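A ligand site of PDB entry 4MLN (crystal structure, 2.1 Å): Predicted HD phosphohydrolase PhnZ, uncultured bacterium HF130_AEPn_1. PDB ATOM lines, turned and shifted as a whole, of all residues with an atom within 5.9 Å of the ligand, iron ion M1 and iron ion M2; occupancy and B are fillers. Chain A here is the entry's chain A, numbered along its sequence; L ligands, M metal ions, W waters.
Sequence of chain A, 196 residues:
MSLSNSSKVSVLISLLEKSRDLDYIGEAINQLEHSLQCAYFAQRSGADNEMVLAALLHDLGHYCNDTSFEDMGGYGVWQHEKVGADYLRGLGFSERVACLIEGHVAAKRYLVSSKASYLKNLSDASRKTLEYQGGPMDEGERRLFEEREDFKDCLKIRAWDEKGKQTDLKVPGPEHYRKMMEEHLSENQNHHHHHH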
ATOM      1  N   ILE A  25     -10.402  22.606  -7.644  1.00  0.00           N
ATOM      2  CA  ILE A  25      -9.755  21.489  -6.940  1.00  0.00           C
ATOM      3  C   ILE A  25     -10.739  20.347  -6.624  1.00  0.00           C
ATOM      4  O   ILE A  25     -10.790  19.824  -5.505  1.00  0.00           O
ATOM      5  CB  ILE A  25      -8.939  21.916  -5.673  1.00  0.00           C
ATOM      6  CG1 ILE A  25      -9.822  22.640  -4.662  1.00  0.00           C
ATOM      7  CG2 ILE A  25      -7.728  22.787  -6.074  1.00  0.00           C
ATOM      8  CD1 ILE A  25      -9.060  23.039  -3.408  1.00  0.00           C
ATOM      9  N   GLU A  27     -13.944  20.167  -6.435  1.00  0.00           N
ATOM     10  CA  GLU A  27     -15.236  20.426  -5.790  1.00  0.00           C
ATOM     11  C   GLU A  27     -16.302  20.976  -6.764  1.00  0.00           C
ATOM     12  O   GLU A  27     -15.975  21.385  -7.889  1.00  0.00           O
ATOM     13  CB  GLU A  27     -15.051  21.349  -4.587  1.00  0.00           C
ATOM     14  CG  GLU A  27     -14.018  20.864  -3.570  1.00  0.00           C
ATOM     15  CD  GLU A  27     -14.570  19.828  -2.570  1.00  0.00           C
ATOM     16  OE1 GLU A  27     -13.912  19.633  -1.514  1.00  0.00           O
ATOM     17  OE2 GLU A  27     -15.640  19.221  -2.821  1.00  0.00           O
ATOM     18  N   HIS A  34     -17.152  28.162  -1.541  1.00  0.00           N
ATOM     19  CA  HIS A  34     -17.018  27.231  -0.432  1.00  0.00           C
ATOM     20  C   HIS A  34     -16.786  27.955   0.907  1.00  0.00           C
ATOM     21  O   HIS A  34     -17.456  27.691   1.897  1.00  0.00           O
ATOM     22  CB  HIS A  34     -15.883  26.226  -0.667  1.00  0.00           C
ATOM     23  CG  HIS A  34     -15.658  25.296   0.483  1.00  0.00           C
ATOM     24  ND1 HIS A  34     -16.675  24.556   1.046  1.00  0.00           N
ATOM     25  CD2 HIS A  34     -14.543  25.002   1.201  1.00  0.00           C
ATOM     26  CE1 HIS A  34     -16.189  23.836   2.057  1.00  0.00           C
ATOM     27  NE2 HIS A  34     -14.900  24.085   2.159  1.00  0.00           N
ATOM     28  N   CYS A  38     -19.632  28.156   4.335  1.00  0.00           N
ATOM     29  CA  CYS A  38     -19.356  27.682   5.684  1.00  0.00           C
ATOM     30  C   CYS A  38     -19.530  28.802   6.706  1.00  0.00           C
ATOM     31  O   CYS A  38     -20.055  28.585   7.799  1.00  0.00           O
ATOM     32  CB  CYS A  38     -17.936  27.100   5.762  1.00  0.00           C
ATOM     33  SG  CYS A  38     -17.663  25.729   4.594  1.00  0.00           S
ATOM     34  N   HIS A  58     -11.153  28.488   6.882  1.00  0.00           N
ATOM     35  CA  HIS A  58     -10.593  27.167   7.130  1.00  0.00           C
ATOM     36  C   HIS A  58      -9.799  26.579   5.961  1.00  0.00           C
ATOM     37  O   HIS A  58      -8.868  25.808   6.183  1.00  0.00           O
ATOM     38  CB  HIS A  58     -11.667  26.171   7.610  1.00  0.00           C
ATOM     39  CG  HIS A  58     -12.448  25.542   6.505  1.00  0.00           C
ATOM     40  ND1 HIS A  58     -13.603  26.105   5.994  1.00  0.00           N
ATOM     41  CD2 HIS A  58     -12.248  24.398   5.812  1.00  0.00           C
ATOM     42  CE1 HIS A  58     -14.075  25.338   5.035  1.00  0.00           C
ATOM     43  NE2 HIS A  58     -13.273  24.291   4.904  1.00  0.00           N
ATOM     44  N   ASP A  59     -10.178  26.921   4.725  1.00  0.00           N
ATOM     45  CA  ASP A  59      -9.443  26.430   3.546  1.00  0.00           C
ATOM     46  C   ASP A  59      -8.508  27.488   2.890  1.00  0.00           C
ATOM     47  O   ASP A  59      -8.098  27.327   1.731  1.00  0.00           O
ATOM     48  CB  ASP A  59     -10.391  25.846   2.500  1.00  0.00           C
ATOM     49  CG  ASP A  59     -10.791  24.419   2.800  1.00  0.00           C
ATOM     50  OD1 ASP A  59     -10.065  23.717   3.553  1.00  0.00           O
ATOM     51  OD2 ASP A  59     -11.818  23.976   2.282  1.00  0.00           O
ATOM     52  N   HIS A  62      -5.106  26.469   0.910  1.00  0.00           N
ATOM     53  CA  HIS A  62      -5.079  25.977  -0.441  1.00  0.00           C
ATOM     54  C   HIS A  62      -4.474  27.043  -1.382  1.00  0.00           C
ATOM     55  O   HIS A  62      -4.129  26.738  -2.531  1.00  0.00           O
ATOM     56  CB  HIS A  62      -6.483  25.585  -0.914  1.00  0.00           C
ATOM     57  CG  HIS A  62      -6.970  24.253  -0.402  1.00  0.00           C
ATOM     58  ND1 HIS A  62      -6.182  23.121  -0.374  1.00  0.00           N
ATOM     59  CD2 HIS A  62      -8.190  23.864   0.050  1.00  0.00           C
ATOM     60  CE1 HIS A  62      -6.880  22.108   0.098  1.00  0.00           C
ATOM     61  NE2 HIS A  62      -8.111  22.519   0.357  1.00  0.00           N
ATOM     62  N   MET A  72      -1.798  17.175  -3.598  1.00  0.00           N
ATOM     63  CA  MET A  72      -2.713  16.111  -3.231  1.00  0.00           C
ATOM     64  C   MET A  72      -3.391  15.618  -4.502  1.00  0.00           C
ATOM     65  O   MET A  72      -4.617  15.498  -4.571  1.00  0.00           O
ATOM     66  CB  MET A  72      -3.714  16.580  -2.165  1.00  0.00           C
ATOM     67  CG  MET A  72      -3.008  17.125  -0.928  1.00  0.00           C
ATOM     68  SD  MET A  72      -3.950  17.095   0.598  1.00  0.00           S
ATOM     69  CE  MET A  72      -5.004  18.542   0.378  1.00  0.00           C
ATOM     70  N   TYR A  75      -6.019  17.833  -5.877  1.00  0.00           N
ATOM     71  CA  TYR A  75      -7.126  18.208  -4.967  1.00  0.00           C
ATOM     72  C   TYR A  75      -6.750  19.115  -3.776  1.00  0.00           C
ATOM     73  O   TYR A  75      -7.483  19.184  -2.791  1.00  0.00           O
ATOM     74  CB  TYR A  75      -7.829  16.957  -4.459  1.00  0.00           C
ATOM     75  CG  TYR A  75      -8.349  16.078  -5.568  1.00  0.00           C
ATOM     76  CD1 TYR A  75      -9.593  16.308  -6.142  1.00  0.00           C
ATOM     77  CD2 TYR A  75      -7.592  15.029  -6.039  1.00  0.00           C
ATOM     78  CE1 TYR A  75     -10.075  15.493  -7.153  1.00  0.00           C
ATOM     79  CE2 TYR A  75      -8.065  14.219  -7.046  1.00  0.00           C
ATOM     80  CZ  TYR A  75      -9.293  14.449  -7.604  1.00  0.00           C
ATOM     81  OH  TYR A  75      -9.746  13.625  -8.612  1.00  0.00           O
ATOM     82  N   HIS A  80      -2.664  22.070   3.820  1.00  0.00           N
ATOM     83  CA  HIS A  80      -3.408  23.323   3.729  1.00  0.00           C
ATOM     84  C   HIS A  80      -3.950  23.786   5.090  1.00  0.00           C
ATOM     85  O   HIS A  80      -3.980  24.976   5.367  1.00  0.00           O
ATOM     86  CB  HIS A  80      -4.534  23.253   2.689  1.00  0.00           C
ATOM     87  CG  HIS A  80      -5.734  22.454   3.138  1.00  0.00           C
ATOM     88  ND1 HIS A  80      -5.706  21.082   3.284  1.00  0.00           N
ATOM     89  CD2 HIS A  80      -7.008  22.829   3.419  1.00  0.00           C
ATOM     90  CE1 HIS A  80      -6.903  20.660   3.656  1.00  0.00           C
ATOM     91  NE2 HIS A  80      -7.710  21.703   3.753  1.00  0.00           N
ATOM     92  N   HIS A 104      -9.369  20.995  11.337  1.00  0.00           N
ATOM     93  CA  HIS A 104     -10.475  20.603  10.465  1.00  0.00           C
ATOM     94  C   HIS A 104     -10.146  19.352   9.661  1.00  0.00           C
ATOM     95  O   HIS A 104     -11.053  18.642   9.230  1.00  0.00           O
ATOM     96  CB  HIS A 104     -11.003  21.778   9.596  1.00  0.00           C
ATOM     97  CG  HIS A 104     -10.328  21.937   8.255  1.00  0.00           C
ATOM     98  ND1 HIS A 104      -9.202  22.722   8.076  1.00  0.00           N
ATOM     99  CD2 HIS A 104     -10.656  21.465   7.033  1.00  0.00           C
ATOM    100  CE1 HIS A 104      -8.861  22.701   6.793  1.00  0.00           C
ATOM    101  NE2 HIS A 104      -9.720  21.947   6.149  1.00  0.00           N
ATOM    102  N   VAL A 105      -8.852  19.065   9.490  1.00  0.00           N
ATOM    103  CA  VAL A 105      -8.446  17.848   8.765  1.00  0.00           C
ATOM    104  C   VAL A 105      -8.426  16.652   9.695  1.00  0.00           C
ATOM    105  O   VAL A 105      -8.939  15.582   9.355  1.00  0.00           O
ATOM    106  CB  VAL A 105      -7.070  17.999   8.045  1.00  0.00           C
ATOM    107  CG1 VAL A 105      -6.556  16.630   7.578  1.00  0.00           C
ATOM    108  CG2 VAL A 105      -7.194  18.964   6.883  1.00  0.00           C
ATOM    109  N   LYS A 108     -11.811  15.319  10.014  1.00  0.00           N
ATOM    110  CA  LYS A 108     -12.178  14.423   8.939  1.00  0.00           C
ATOM    111  C   LYS A 108     -11.616  13.024   9.191  1.00  0.00           C
ATOM    112  O   LYS A 108     -12.300  12.019   8.990  1.00  0.00           O
ATOM    113  CB  LYS A 108     -11.651  14.936   7.591  1.00  0.00           C
ATOM    114  CG  LYS A 108     -12.362  14.336   6.397  1.00  0.00           C
ATOM    115  CD  LYS A 108     -11.451  14.012   5.214  1.00  0.00           C
ATOM    116  CE  LYS A 108     -10.430  15.088   4.942  1.00  0.00           C
ATOM    117  NZ  LYS A 108      -9.889  14.987   3.547  1.00  0.00           N
ATOM    118  N   SER A 123     -17.218  14.488   0.034  1.00  0.00           N
ATOM    119  CA  SER A 123     -17.120  14.820  -1.384  1.00  0.00           C
ATOM    120  C   SER A 123     -16.039  13.927  -1.984  1.00  0.00           C
ATOM    121  O   SER A 123     -15.233  13.375  -1.250  1.00  0.00           O
ATOM    122  CB  SER A 123     -16.775  16.297  -1.583  1.00  0.00           C
ATOM    123  OG  SER A 123     -15.455  16.581  -1.149  1.00  0.00           O
ATOM    124  N   ALA A 125     -13.513  14.859  -3.702  1.00  0.00           N
ATOM    125  CA  ALA A 125     -12.242  15.507  -3.401  1.00  0.00           C
ATOM    126  C   ALA A 125     -11.755  15.159  -1.985  1.00  0.00           C
ATOM    127  O   ALA A 125     -10.589  14.820  -1.792  1.00  0.00           O
ATOM    128  CB  ALA A 125     -12.345  17.028  -3.603  1.00  0.00           C
ATOM    129  N   SER A 126     -12.638  15.224  -0.996  1.00  0.00           N
ATOM    130  CA  SER A 126     -12.222  15.029   0.398  1.00  0.00           C
ATOM    131  C   SER A 126     -11.735  13.611   0.692  1.00  0.00           C
ATOM    132  O   SER A 126     -10.711  13.419   1.363  1.00  0.00           O
ATOM    133  CB  SER A 126     -13.324  15.443   1.379  1.00  0.00           C
ATOM    134  OG  SER A 126     -13.419  16.858   1.460  1.00  0.00           O
ATOM    135  N   THR A 129      -8.217  13.362  -0.602  1.00  0.00           N
ATOM    136  CA  THR A 129      -7.160  14.077   0.108  1.00  0.00           C
ATOM    137  C   THR A 129      -6.781  13.365   1.385  1.00  0.00           C
ATOM    138  O   THR A 129      -5.654  13.483   1.855  1.00  0.00           O
ATOM    139  CB  THR A 129      -7.537  15.537   0.415  1.00  0.00           C
ATOM    140  OG1 THR A 129      -8.738  15.556   1.178  1.00  0.00           O
ATOM    141  CG2 THR A 129      -7.726  16.327  -0.875  1.00  0.00           C
ATOM    142  N   LEU A 130      -7.715  12.595   1.940  1.00  0.00           N
ATOM    143  CA  LEU A 130      -7.439  11.804   3.136  1.00  0.00           C
ATOM    144  C   LEU A 130      -6.138  10.960   2.993  1.00  0.00           C
ATOM    145  O   LEU A 130      -5.479  10.675   3.995  1.00  0.00           O
ATOM    146  CB  LEU A 130      -8.617  10.888   3.426  1.00  0.00           C
ATOM    147  CG  LEU A 130      -8.671  10.178   4.786  1.00  0.00           C
ATOM    148  CD1 LEU A 130      -8.601  11.175   5.943  1.00  0.00           C
ATOM    149  CD2 LEU A 130      -9.946   9.331   4.905  1.00  0.00           C
ATOM    150  N   GLN A 133      -3.066  12.884   3.970  1.00  0.00           N
ATOM    151  CA  GLN A 133      -3.245  13.526   5.270  1.00  0.00           C
ATOM    152  C   GLN A 133      -3.011  12.577   6.444  1.00  0.00           C
ATOM    153  O   GLN A 133      -3.133  12.963   7.611  1.00  0.00           O
ATOM    154  CB  GLN A 133      -4.641  14.183   5.332  1.00  0.00           C
ATOM    155  CG  GLN A 133      -4.761  15.351   4.361  1.00  0.00           C
ATOM    156  CD  GLN A 133      -6.195  15.811   4.078  1.00  0.00           C
ATOM    157  OE1 GLN A 133      -7.159  15.072   4.211  1.00  0.00           O
ATOM    158  NE2 GLN A 133      -6.311  17.067   3.647  1.00  0.00           N
ATOM    159  N   ARG A 158     -16.109  21.051  10.975  1.00  0.00           N
ATOM    160  CA  ARG A 158     -16.053  20.044   9.919  1.00  0.00           C
ATOM    161  C   ARG A 158     -17.434  19.807   9.318  1.00  0.00           C
ATOM    162  O   ARG A 158     -17.578  19.602   8.095  1.00  0.00           O
ATOM    163  CB  ARG A 158     -15.402  18.752  10.416  1.00  0.00           C
ATOM    164  CG  ARG A 158     -15.012  17.792   9.321  1.00  0.00           C
ATOM    165  CD  ARG A 158     -13.903  18.347   8.463  1.00  0.00           C
ATOM    166  NE  ARG A 158     -14.042  17.935   7.060  1.00  0.00           N
ATOM    167  CZ  ARG A 158     -13.066  18.040   6.148  1.00  0.00           C
ATOM    168  NH1 ARG A 158     -11.879  18.514   6.500  1.00  0.00           N
ATOM    169  NH2 ARG A 158     -13.290  17.658   4.900  1.00  0.00           N
ATOM    170  N   ASP A 161     -18.193  22.372   6.942  1.00  0.00           N
ATOM    171  CA  ASP A 161     -17.262  22.183   5.845  1.00  0.00           C
ATOM    172  C   ASP A 161     -17.910  21.229   4.839  1.00  0.00           C
ATOM    173  O   ASP A 161     -17.950  21.529   3.644  1.00  0.00           O
ATOM    174  CB  ASP A 161     -15.940  21.610   6.381  1.00  0.00           C
ATOM    175  CG  ASP A 161     -14.846  21.528   5.318  1.00  0.00           C
ATOM    176  OD1 ASP A 161     -14.973  22.115   4.233  1.00  0.00           O
ATOM    177  OD2 ASP A 161     -13.821  20.878   5.594  1.00  0.00           O
ATOM    178  N   GLU A 162     -18.437  20.104   5.313  1.00  0.00           N
ATOM    179  CA  GLU A 162     -19.053  19.148   4.391  1.00  0.00           C
ATOM    180  C   GLU A 162     -20.350  19.705   3.777  1.00  0.00           C
ATOM    181  O   GLU A 162     -20.763  19.277   2.696  1.00  0.00           O
ATOM    182  CB  GLU A 162     -19.327  17.797   5.064  1.00  0.00           C
ATOM    183  CG  GLU A 162     -18.343  17.403   6.153  1.00  0.00           C
ATOM    184  CD  GLU A 162     -16.963  17.029   5.645  1.00  0.00           C
ATOM    185  OE1 GLU A 162     -16.726  16.959   4.417  1.00  0.00           O
ATOM    186  OE2 GLU A 162     -16.088  16.805   6.510  1.00  0.00           O
HETATM  187  O1  LIG L   1      -9.038  17.990   2.603  1.00  0.00           O
HETATM  188  P1  LIG L   1     -10.291  18.728   2.953  1.00  0.00           P
HETATM  189  O2  LIG L   1      -9.991  19.328   4.286  1.00  0.00           O
HETATM  190  O3  LIG L   1     -11.306  17.652   3.164  1.00  0.00           O
HETATM  191  C1  LIG L   1     -10.851  19.929   1.715  1.00  0.00           C
HETATM  192  O4  LIG L   1     -10.152  21.105   1.881  1.00  0.00           O
HETATM  193  C2  LIG L   1     -10.654  19.332   0.359  1.00  0.00           C
HETATM  194  N1  LIG L   1     -11.210  20.191  -0.659  1.00  0.00           N
HETATM  195 FE    FE M   1     -13.338  22.978   3.299  1.00  0.00          FE
HETATM  196 FE    FE M   2      -9.938  21.614   4.036  1.00  0.00          FE
HETATM  197  O   HOH W   1     -13.455  21.613   1.655  1.00  0.00           O
HETATM  198  O   HOH W   2     -11.996  21.642   4.188  1.00  0.00           O
HETATM  199  O   HOH W   3     -11.332  22.904  -0.228  1.00  0.00           O
HETATM  200  O   HOH W   4      -9.980  19.343  -3.007  1.00  0.00           O
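Iron ion M2 is bound by water W2, a ring nitrogen (NE2) of His 104, the side-chain carboxylate (OD1) of Asp 59, an oxygen (O4) of the ligand, a ring nitrogen (NE2) of His 80 and an oxygen (O2) of the ligand.
The side-chain carboxylate (OD1) of Asp 161 is bound to iron ion M1 (2.1 Å). A ring nitrogen (NE2) of His 58 is bound to iron ion M1, at 2.1 Å. OD2 of Asp 59 binds iron ion M1, 2.1 Å away. Iron ion M1 is bound by water W2 (2.1 Å). Water W1 binds iron ion M1. Iron ion M1 is bound by a ring nitrogen (NE2) of His 34. Iron ion M1 has six donor atoms within binding distance.
CG2 of Val 105 touches O2 of the ligand, 3.8 Å away. Along chain A the residues within 4 Å of the ligand span positions 27 to 158. The nearest printed residue that does not touch the ligand is Asp 161 (4.3 Å).
A nitrogen (N1) of the ligand is in salt-bridge range of the side-chain carboxylate (OE1) of Glu 27 (2.9 Å). NE2 of Gln 133 is in hydrogen-bond range of O1 of the ligand (3.1 Å). O1 of the ligand lies within hydrogen-bond range of OG1 of Thr 129 (2.8 Å). The side-chain amino group (NZ) of Lys 108 is in salt-bridge range of an oxygen (O3) of the ligand (3.0 Å). NH2 of Arg 158 is in salt-bridge range of O3 of the ligand (2.6 Å). NE2 of His 62 lies close to O4 of the ligand (2.9 Å). OG of Ser 126 is in hydrogen-bond range of O3 of the ligand (2.8 Å).
Within 4 Å of iron ion M1: His 34, His 58, Asp 59 and Asp 161.
O of Ser 126 is in hydrogen-bond range of NZ of Lys 108 (2.8 Å). The backbone carbonyl oxygen (O) of Thr 129 lies close to the side-chain amide oxygen (OE1) of Gln 133, 3.2 Å away. The side-chain amino group (NZ) of Lys 108 is in hydrogen-bond range of the side-chain amide oxygen (OE1) of Gln 133 (2.8 Å). The side-chain hydroxyl of Ser 123 lies within hydrogen-bond range of the side-chain carboxylate of Glu 27 (3.1 Å). OG1 of Thr 129 is in hydrogen-bond range of O of Ser 126 (2.9 Å). The side-chain carboxylate (OE2) of Glu 162 is in salt-bridge range of the guanidinium group (NE) of Arg 158, at 2.4 Å. O of His 104 sits at hydrogen-bond distance from NH1 of Arg 158, at 2.9 Å. OE1 of Gln 133 is in hydrogen-bond range of N of Leu 130, at 3.4 Å.
Water W3 lies within hydrogen-bond range of N1 of the ligand (2.7 Å) and NE2 of His 62 (3.3 Å). Water W4 lies within hydrogen-bond range of the backbone carbonyl oxygen (O) of Tyr 75, the backbone carbonyl oxygen (O) of Ile 25 and a nitrogen (N1) of the ligand.
Of the 22 residues printed, 3 come within 4 Å of iron ion M2. Along chain A the residues within 4 Å of iron ion M2 span positions 59 to 104.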
